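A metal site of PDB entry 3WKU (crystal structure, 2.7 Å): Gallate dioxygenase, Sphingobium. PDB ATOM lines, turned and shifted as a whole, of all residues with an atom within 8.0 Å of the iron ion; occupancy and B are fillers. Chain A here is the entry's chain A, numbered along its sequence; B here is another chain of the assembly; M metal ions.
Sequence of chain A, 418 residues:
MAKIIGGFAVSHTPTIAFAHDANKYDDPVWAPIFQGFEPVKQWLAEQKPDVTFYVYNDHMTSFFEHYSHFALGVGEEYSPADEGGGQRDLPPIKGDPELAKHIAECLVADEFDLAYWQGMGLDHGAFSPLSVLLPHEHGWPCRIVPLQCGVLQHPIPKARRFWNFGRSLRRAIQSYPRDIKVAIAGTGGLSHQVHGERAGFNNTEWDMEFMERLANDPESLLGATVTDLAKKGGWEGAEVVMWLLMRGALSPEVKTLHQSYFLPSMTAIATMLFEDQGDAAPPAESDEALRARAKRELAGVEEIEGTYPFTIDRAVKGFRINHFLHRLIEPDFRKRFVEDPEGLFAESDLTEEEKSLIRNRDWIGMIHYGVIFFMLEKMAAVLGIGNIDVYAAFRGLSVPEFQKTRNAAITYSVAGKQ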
ATOM      1  N   SER A  11     -30.686  -9.812 -11.630  1.00  0.00           N
ATOM      2  CA  SER A  11     -30.834  -9.500 -13.056  1.00  0.00           C
ATOM      3  C   SER A  11     -31.688  -8.249 -13.266  1.00  0.00           C
ATOM      4  O   SER A  11     -32.573  -7.969 -12.453  1.00  0.00           O
ATOM      5  CB  SER A  11     -31.475 -10.671 -13.801  1.00  0.00           C
ATOM      6  OG  SER A  11     -30.512 -11.621 -14.189  1.00  0.00           O
ATOM      7  N   HIS A  12     -31.428  -7.504 -14.342  1.00  0.00           N
ATOM      8  CA  HIS A  12     -32.214  -6.301 -14.638  1.00  0.00           C
ATOM      9  C   HIS A  12     -32.850  -6.271 -16.031  1.00  0.00           C
ATOM     10  O   HIS A  12     -33.220  -5.203 -16.526  1.00  0.00           O
ATOM     11  CB  HIS A  12     -31.441  -4.997 -14.316  1.00  0.00           C
ATOM     12  CG  HIS A  12     -30.096  -4.887 -14.982  1.00  0.00           C
ATOM     13  ND1 HIS A  12     -28.958  -5.481 -14.471  1.00  0.00           N
ATOM     14  CD2 HIS A  12     -29.709  -4.234 -16.105  1.00  0.00           C
ATOM     15  CE1 HIS A  12     -27.933  -5.207 -15.257  1.00  0.00           C
ATOM     16  NE2 HIS A  12     -28.362  -4.448 -16.257  1.00  0.00           N
ATOM     17  N   THR A  13     -33.001  -7.446 -16.648  1.00  0.00           N
ATOM     18  CA  THR A  13     -33.541  -7.557 -18.002  1.00  0.00           C
ATOM     19  C   THR A  13     -34.943  -6.962 -18.093  1.00  0.00           C
ATOM     20  O   THR A  13     -35.796  -7.266 -17.247  1.00  0.00           O
ATOM     21  CB  THR A  13     -33.571  -9.019 -18.478  1.00  0.00           C
ATOM     22  OG1 THR A  13     -32.419  -9.726 -17.975  1.00  0.00           O
ATOM     23  CG2 THR A  13     -33.618  -9.108 -20.007  1.00  0.00           C
ATOM     24  N   PRO A  14     -35.195  -6.126 -19.122  1.00  0.00           N
ATOM     25  CA  PRO A  14     -36.495  -5.478 -19.255  1.00  0.00           C
ATOM     26  C   PRO A  14     -37.592  -6.442 -19.687  1.00  0.00           C
ATOM     27  O   PRO A  14     -38.693  -6.015 -20.006  1.00  0.00           O
ATOM     28  CB  PRO A  14     -36.243  -4.432 -20.346  1.00  0.00           C
ATOM     29  CG  PRO A  14     -35.214  -5.042 -21.189  1.00  0.00           C
ATOM     30  CD  PRO A  14     -34.304  -5.774 -20.238  1.00  0.00           C
ATOM     31  N   TYR A  56     -26.657   0.030 -10.780  1.00  0.00           N
ATOM     32  CA  TYR A  56     -27.098  -0.433 -12.077  1.00  0.00           C
ATOM     33  C   TYR A  56     -26.224   0.158 -13.186  1.00  0.00           C
ATOM     34  O   TYR A  56     -25.325   0.958 -12.927  1.00  0.00           O
ATOM     35  CB  TYR A  56     -28.542   0.018 -12.287  1.00  0.00           C
ATOM     36  CG  TYR A  56     -28.648   1.467 -12.654  1.00  0.00           C
ATOM     37  CD1 TYR A  56     -29.010   1.842 -13.939  1.00  0.00           C
ATOM     38  CD2 TYR A  56     -28.337   2.460 -11.732  1.00  0.00           C
ATOM     39  CE1 TYR A  56     -29.091   3.165 -14.301  1.00  0.00           C
ATOM     40  CE2 TYR A  56     -28.422   3.796 -12.078  1.00  0.00           C
ATOM     41  CZ  TYR A  56     -28.796   4.137 -13.365  1.00  0.00           C
ATOM     42  OH  TYR A  56     -28.877   5.460 -13.726  1.00  0.00           O
ATOM     43  N   ASN A  57     -26.492  -0.244 -14.433  1.00  0.00           N
ATOM     44  CA  ASN A  57     -25.920   0.433 -15.592  1.00  0.00           C
ATOM     45  C   ASN A  57     -26.997   1.034 -16.479  1.00  0.00           C
ATOM     46  O   ASN A  57     -27.972   0.358 -16.824  1.00  0.00           O
ATOM     47  CB  ASN A  57     -24.959  -0.478 -16.375  1.00  0.00           C
ATOM     48  CG  ASN A  57     -25.622  -1.202 -17.527  1.00  0.00           C
ATOM     49  OD1 ASN A  57     -26.310  -2.208 -17.354  1.00  0.00           O
ATOM     50  ND2 ASN A  57     -25.395  -0.696 -18.732  1.00  0.00           N
ATOM     51  N   ASP A  58     -26.873   2.317 -16.803  1.00  0.00           N
ATOM     52  CA  ASP A  58     -27.664   2.911 -17.858  1.00  0.00           C
ATOM     53  C   ASP A  58     -27.250   2.238 -19.181  1.00  0.00           C
ATOM     54  O   ASP A  58     -26.069   1.968 -19.412  1.00  0.00           O
ATOM     55  CB  ASP A  58     -27.412   4.415 -17.891  1.00  0.00           C
ATOM     56  CG  ASP A  58     -28.272   5.150 -18.910  1.00  0.00           C
ATOM     57  OD1 ASP A  58     -28.983   6.081 -18.489  1.00  0.00           O
ATOM     58  OD2 ASP A  58     -28.221   4.818 -20.127  1.00  0.00           O
ATOM     59  N   HIS A  59     -28.227   1.952 -20.042  1.00  0.00           N
ATOM     60  CA  HIS A  59     -27.930   1.272 -21.311  1.00  0.00           C
ATOM     61  C   HIS A  59     -28.052   2.236 -22.492  1.00  0.00           C
ATOM     62  O   HIS A  59     -28.952   2.099 -23.337  1.00  0.00           O
ATOM     63  CB  HIS A  59     -28.841   0.043 -21.494  1.00  0.00           C
ATOM     64  CG  HIS A  59     -28.760  -0.953 -20.366  1.00  0.00           C
ATOM     65  ND1 HIS A  59     -29.386  -0.750 -19.148  1.00  0.00           N
ATOM     66  CD2 HIS A  59     -28.164  -2.162 -20.291  1.00  0.00           C
ATOM     67  CE1 HIS A  59     -29.155  -1.788 -18.370  1.00  0.00           C
ATOM     68  NE2 HIS A  59     -28.416  -2.658 -19.035  1.00  0.00           N
ATOM     69  N   ASP A 123     -33.170   4.196 -16.577  1.00  0.00           N
ATOM     70  CA  ASP A 123     -33.418   3.218 -17.641  1.00  0.00           C
ATOM     71  C   ASP A 123     -33.799   1.849 -17.089  1.00  0.00           C
ATOM     72  O   ASP A 123     -33.888   1.676 -15.860  1.00  0.00           O
ATOM     73  CB  ASP A 123     -32.251   3.176 -18.656  1.00  0.00           C
ATOM     74  CG  ASP A 123     -31.231   2.052 -18.387  1.00  0.00           C
ATOM     75  OD1 ASP A 123     -30.856   1.802 -17.216  1.00  0.00           O
ATOM     76  OD2 ASP A 123     -30.787   1.438 -19.390  1.00  0.00           O
ATOM     77  N   HIS A 124     -34.022   0.880 -17.981  1.00  0.00           N
ATOM     78  CA  HIS A 124     -34.374  -0.482 -17.601  1.00  0.00           C
ATOM     79  C   HIS A 124     -33.406  -1.071 -16.580  1.00  0.00           C
ATOM     80  O   HIS A 124     -33.784  -1.946 -15.816  1.00  0.00           O
ATOM     81  CB  HIS A 124     -34.491  -1.377 -18.845  1.00  0.00           C
ATOM     82  CG  HIS A 124     -33.224  -2.095 -19.224  1.00  0.00           C
ATOM     83  ND1 HIS A 124     -32.578  -1.875 -20.431  1.00  0.00           N
ATOM     84  CD2 HIS A 124     -32.489  -3.034 -18.575  1.00  0.00           C
ATOM     85  CE1 HIS A 124     -31.511  -2.650 -20.496  1.00  0.00           C
ATOM     86  NE2 HIS A 124     -31.425  -3.361 -19.392  1.00  0.00           N
ATOM     87  N   GLY A 125     -32.166  -0.605 -16.572  1.00  0.00           N
ATOM     88  CA  GLY A 125     -31.163  -1.116 -15.648  1.00  0.00           C
ATOM     89  C   GLY A 125     -31.603  -0.919 -14.212  1.00  0.00           C
ATOM     90  O   GLY A 125     -31.162  -1.644 -13.318  1.00  0.00           O
ATOM     91  N   VAL A 151     -19.922   0.540 -18.174  1.00  0.00           N
ATOM     92  CA  VAL A 151     -19.431  -0.819 -18.364  1.00  0.00           C
ATOM     93  C   VAL A 151     -19.516  -1.254 -19.826  1.00  0.00           C
ATOM     94  O   VAL A 151     -19.067  -2.336 -20.193  1.00  0.00           O
ATOM     95  CB  VAL A 151     -20.185  -1.823 -17.462  1.00  0.00           C
ATOM     96  CG1 VAL A 151     -19.903  -1.538 -15.993  1.00  0.00           C
ATOM     97  CG2 VAL A 151     -21.695  -1.785 -17.743  1.00  0.00           C
ATOM     98  N   LEU A 152     -20.073  -0.376 -20.654  1.00  0.00           N
ATOM     99  CA  LEU A 152     -20.291  -0.655 -22.084  1.00  0.00           C
ATOM    100  C   LEU A 152     -19.176  -0.079 -22.992  1.00  0.00           C
ATOM    101  O   LEU A 152     -18.992  -0.548 -24.124  1.00  0.00           O
ATOM    102  CB  LEU A 152     -21.667  -0.108 -22.502  1.00  0.00           C
ATOM    103  CG  LEU A 152     -22.865  -0.403 -21.573  1.00  0.00           C
ATOM    104  CD1 LEU A 152     -23.989   0.622 -21.721  1.00  0.00           C
ATOM    105  CD2 LEU A 152     -23.397  -1.838 -21.743  1.00  0.00           C
ATOM    106  N   THR A 187     -27.598  -4.499  -9.036  1.00  0.00           N
ATOM    107  CA  THR A 187     -28.318  -5.120 -10.132  1.00  0.00           C
ATOM    108  C   THR A 187     -27.464  -5.362 -11.373  1.00  0.00           C
ATOM    109  O   THR A 187     -27.189  -4.441 -12.138  1.00  0.00           O
ATOM    110  CB  THR A 187     -29.570  -4.310 -10.522  1.00  0.00           C
ATOM    111  OG1 THR A 187     -29.195  -3.148 -11.274  1.00  0.00           O
ATOM    112  CG2 THR A 187     -30.324  -3.870  -9.272  1.00  0.00           C
ATOM    113  N   GLY A 188     -27.059  -6.614 -11.556  1.00  0.00           N
ATOM    114  CA  GLY A 188     -26.302  -6.995 -12.734  1.00  0.00           C
ATOM    115  C   GLY A 188     -26.586  -8.406 -13.217  1.00  0.00           C
ATOM    116  O   GLY A 188     -26.974  -9.275 -12.434  1.00  0.00           O
ATOM    117  N   GLY A 189     -26.397  -8.611 -14.515  1.00  0.00           N
ATOM    118  CA  GLY A 189     -26.385  -9.950 -15.096  1.00  0.00           C
ATOM    119  C   GLY A 189     -27.738 -10.611 -15.212  1.00  0.00           C
ATOM    120  O   GLY A 189     -28.759  -9.930 -15.349  1.00  0.00           O
ATOM    121  N   LEU A 190     -27.745 -11.953 -15.193  1.00  0.00           N
ATOM    122  CA  LEU A 190     -26.510 -12.743 -15.159  1.00  0.00           C
ATOM    123  C   LEU A 190     -26.034 -13.030 -16.589  1.00  0.00           C
ATOM    124  O   LEU A 190     -26.421 -12.310 -17.517  1.00  0.00           O
ATOM    125  CB  LEU A 190     -26.710 -14.037 -14.353  1.00  0.00           C
ATOM    126  CG  LEU A 190     -25.614 -14.422 -13.348  1.00  0.00           C
ATOM    127  CD1 LEU A 190     -26.147 -15.469 -12.375  1.00  0.00           C
ATOM    128  CD2 LEU A 190     -24.312 -14.894 -14.017  1.00  0.00           C
ATOM    129  N   HIS A 192     -25.111 -13.580 -20.305  1.00  0.00           N
ATOM    130  CA  HIS A 192     -25.842 -13.420 -21.581  1.00  0.00           C
ATOM    131  C   HIS A 192     -25.024 -12.635 -22.600  1.00  0.00           C
ATOM    132  O   HIS A 192     -23.935 -12.127 -22.283  1.00  0.00           O
ATOM    133  CB  HIS A 192     -27.220 -12.746 -21.370  1.00  0.00           C
ATOM    134  CG  HIS A 192     -27.162 -11.325 -20.906  1.00  0.00           C
ATOM    135  ND1 HIS A 192     -26.419 -10.917 -19.812  1.00  0.00           N
ATOM    136  CD2 HIS A 192     -27.775 -10.215 -21.370  1.00  0.00           C
ATOM    137  CE1 HIS A 192     -26.577  -9.623 -19.635  1.00  0.00           C
ATOM    138  NE2 HIS A 192     -27.399  -9.166 -20.571  1.00  0.00           N
ATOM    139  N   VAL A 194     -26.256 -10.029 -26.062  1.00  0.00           N
ATOM    140  CA  VAL A 194     -27.419  -9.536 -26.802  1.00  0.00           C
ATOM    141  C   VAL A 194     -27.064  -8.919 -28.144  1.00  0.00           C
ATOM    142  O   VAL A 194     -27.929  -8.382 -28.851  1.00  0.00           O
ATOM    143  CB  VAL A 194     -28.271  -8.505 -25.970  1.00  0.00           C
ATOM    144  CG1 VAL A 194     -28.891  -9.152 -24.730  1.00  0.00           C
ATOM    145  CG2 VAL A 194     -27.458  -7.279 -25.597  1.00  0.00           C
ATOM    146  N   GLU A 236     -22.132  -8.898 -22.785  1.00  0.00           N
ATOM    147  CA  GLU A 236     -22.911  -8.050 -21.899  1.00  0.00           C
ATOM    148  C   GLU A 236     -22.998  -8.669 -20.520  1.00  0.00           C
ATOM    149  O   GLU A 236     -23.136  -7.945 -19.524  1.00  0.00           O
ATOM    150  CB  GLU A 236     -24.301  -7.824 -22.465  1.00  0.00           C
ATOM    151  CG  GLU A 236     -24.379  -6.746 -23.527  1.00  0.00           C
ATOM    152  CD  GLU A 236     -23.885  -7.228 -24.895  1.00  0.00           C
ATOM    153  OE1 GLU A 236     -24.191  -8.389 -25.273  1.00  0.00           O
ATOM    154  OE2 GLU A 236     -23.223  -6.425 -25.586  1.00  0.00           O
ATOM    155  N   GLY A 237     -22.887  -9.987 -20.462  1.00  0.00           N
ATOM    156  CA  GLY A 237     -23.007 -10.754 -19.222  1.00  0.00           C
ATOM    157  C   GLY A 237     -21.946 -10.406 -18.215  1.00  0.00           C
ATOM    158  O   GLY A 237     -22.134 -10.595 -17.013  1.00  0.00           O
ATOM    159  N   GLU A 239     -21.273  -7.541 -17.257  1.00  0.00           N
ATOM    160  CA  GLU A 239     -21.763  -6.458 -16.395  1.00  0.00           C
ATOM    161  C   GLU A 239     -21.888  -6.894 -14.926  1.00  0.00           C
ATOM    162  O   GLU A 239     -22.298  -6.126 -14.057  1.00  0.00           O
ATOM    163  CB  GLU A 239     -23.081  -5.880 -16.916  1.00  0.00           C
ATOM    164  CG  GLU A 239     -24.321  -6.742 -16.658  1.00  0.00           C
ATOM    165  CD  GLU A 239     -25.611  -6.112 -17.175  1.00  0.00           C
ATOM    166  OE1 GLU A 239     -25.703  -4.857 -17.201  1.00  0.00           O
ATOM    167  OE2 GLU A 239     -26.541  -6.861 -17.539  1.00  0.00           O
ATOM    168  N   MET A 242     -20.651  -5.317 -11.377  1.00  0.00           N
ATOM    169  CA  MET A 242     -21.513  -4.532 -10.487  1.00  0.00           C
ATOM    170  C   MET A 242     -21.979  -5.312  -9.239  1.00  0.00           C
ATOM    171  O   MET A 242     -22.472  -4.706  -8.283  1.00  0.00           O
ATOM    172  CB  MET A 242     -22.734  -4.020 -11.260  1.00  0.00           C
ATOM    173  CG  MET A 242     -22.459  -2.863 -12.197  1.00  0.00           C
ATOM    174  SD  MET A 242     -23.999  -2.057 -12.718  1.00  0.00           S
ATOM    175  CE  MET A 242     -24.661  -3.295 -13.826  1.00  0.00           C
ATOM    176  N   THR A 267     -31.946 -13.750 -21.687  1.00  0.00           N
ATOM    177  CA  THR A 267     -31.034 -13.473 -20.609  1.00  0.00           C
ATOM    178  C   THR A 267     -31.271 -14.429 -19.469  1.00  0.00           C
ATOM    179  O   THR A 267     -32.416 -14.735 -19.145  1.00  0.00           O
ATOM    180  CB  THR A 267     -31.248 -12.037 -20.100  1.00  0.00           C
ATOM    181  OG1 THR A 267     -31.337 -11.132 -21.207  1.00  0.00           O
ATOM    182  CG2 THR A 267     -30.132 -11.606 -19.161  1.00  0.00           C
ATOM    183  N   PHE B 374     -27.956  -1.382 -27.760  1.00  0.00           N
ATOM    184  CA  PHE B 374     -28.974  -0.661 -27.034  1.00  0.00           C
ATOM    185  C   PHE B 374     -29.530   0.510 -27.815  1.00  0.00           C
ATOM    186  O   PHE B 374     -30.563   1.054 -27.466  1.00  0.00           O
ATOM    187  CB  PHE B 374     -28.418  -0.258 -25.681  1.00  0.00           C
ATOM    188  CG  PHE B 374     -27.966  -1.428 -24.864  1.00  0.00           C
ATOM    189  CD1 PHE B 374     -28.892  -2.329 -24.338  1.00  0.00           C
ATOM    190  CD2 PHE B 374     -26.619  -1.673 -24.655  1.00  0.00           C
ATOM    191  CE1 PHE B 374     -28.495  -3.420 -23.589  1.00  0.00           C
ATOM    192  CE2 PHE B 374     -26.204  -2.776 -23.904  1.00  0.00           C
ATOM    193  CZ  PHE B 374     -27.140  -3.642 -23.358  1.00  0.00           C
ATOM    194  N   GLU B 377     -32.107  -1.654 -29.815  1.00  0.00           N
ATOM    195  CA  GLU B 377     -33.152  -2.012 -28.857  1.00  0.00           C
ATOM    196  C   GLU B 377     -34.162  -0.864 -28.730  1.00  0.00           C
ATOM    197  O   GLU B 377     -35.373  -1.093 -28.728  1.00  0.00           O
ATOM    198  CB  GLU B 377     -32.556  -2.329 -27.502  1.00  0.00           C
ATOM    199  CG  GLU B 377     -33.543  -2.869 -26.481  1.00  0.00           C
ATOM    200  CD  GLU B 377     -32.840  -3.447 -25.263  1.00  0.00           C
ATOM    201  OE1 GLU B 377     -31.607  -3.629 -25.299  1.00  0.00           O
ATOM    202  OE2 GLU B 377     -33.515  -3.730 -24.251  1.00  0.00           O
HETATM  203 FE    FE M   1     -27.548  -4.581 -18.604  1.00  0.00          FE
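Merely in contact with the iron ion: Asn 57 (3.0 Å).
The iron ion is bound by NE2 of His 59 (2.2 Å). The iron ion is bound by the side-chain carboxylate (OE1) of Glu 239. The iron ion is bound by NE2 of His 12 (2.5 Å). Slightly farther from the iron ion lies OE2 of Glu 239 (2.7 Å).
O of Asn 57 lies close to ND1 of His 59 (2.9 Å). ND1 of His 59 lies close to NE2 of His 124 (3.3 Å). A ring nitrogen (ND1) of His 59 lies within hydrogen-bond range of the side-chain carboxylate of Asp 123 (2.6 Å). OE1 of Glu 239 lies close to OD1 of Asn 57, 2.7 Å away. The side-chain carboxylate (OE2) of Glu 239 sits at hydrogen-bond distance from the backbone NH (N) of Gly 189 (3.5 Å). NE2 of His 12 sits close to OD1 of Asn 57. O of Thr 187 is in hydrogen-bond range of ND1 of His 12. The backbone NH of Asn 57 sits at hydrogen-bond distance from the side-chain sulfur of Met 242 (3.5 Å).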
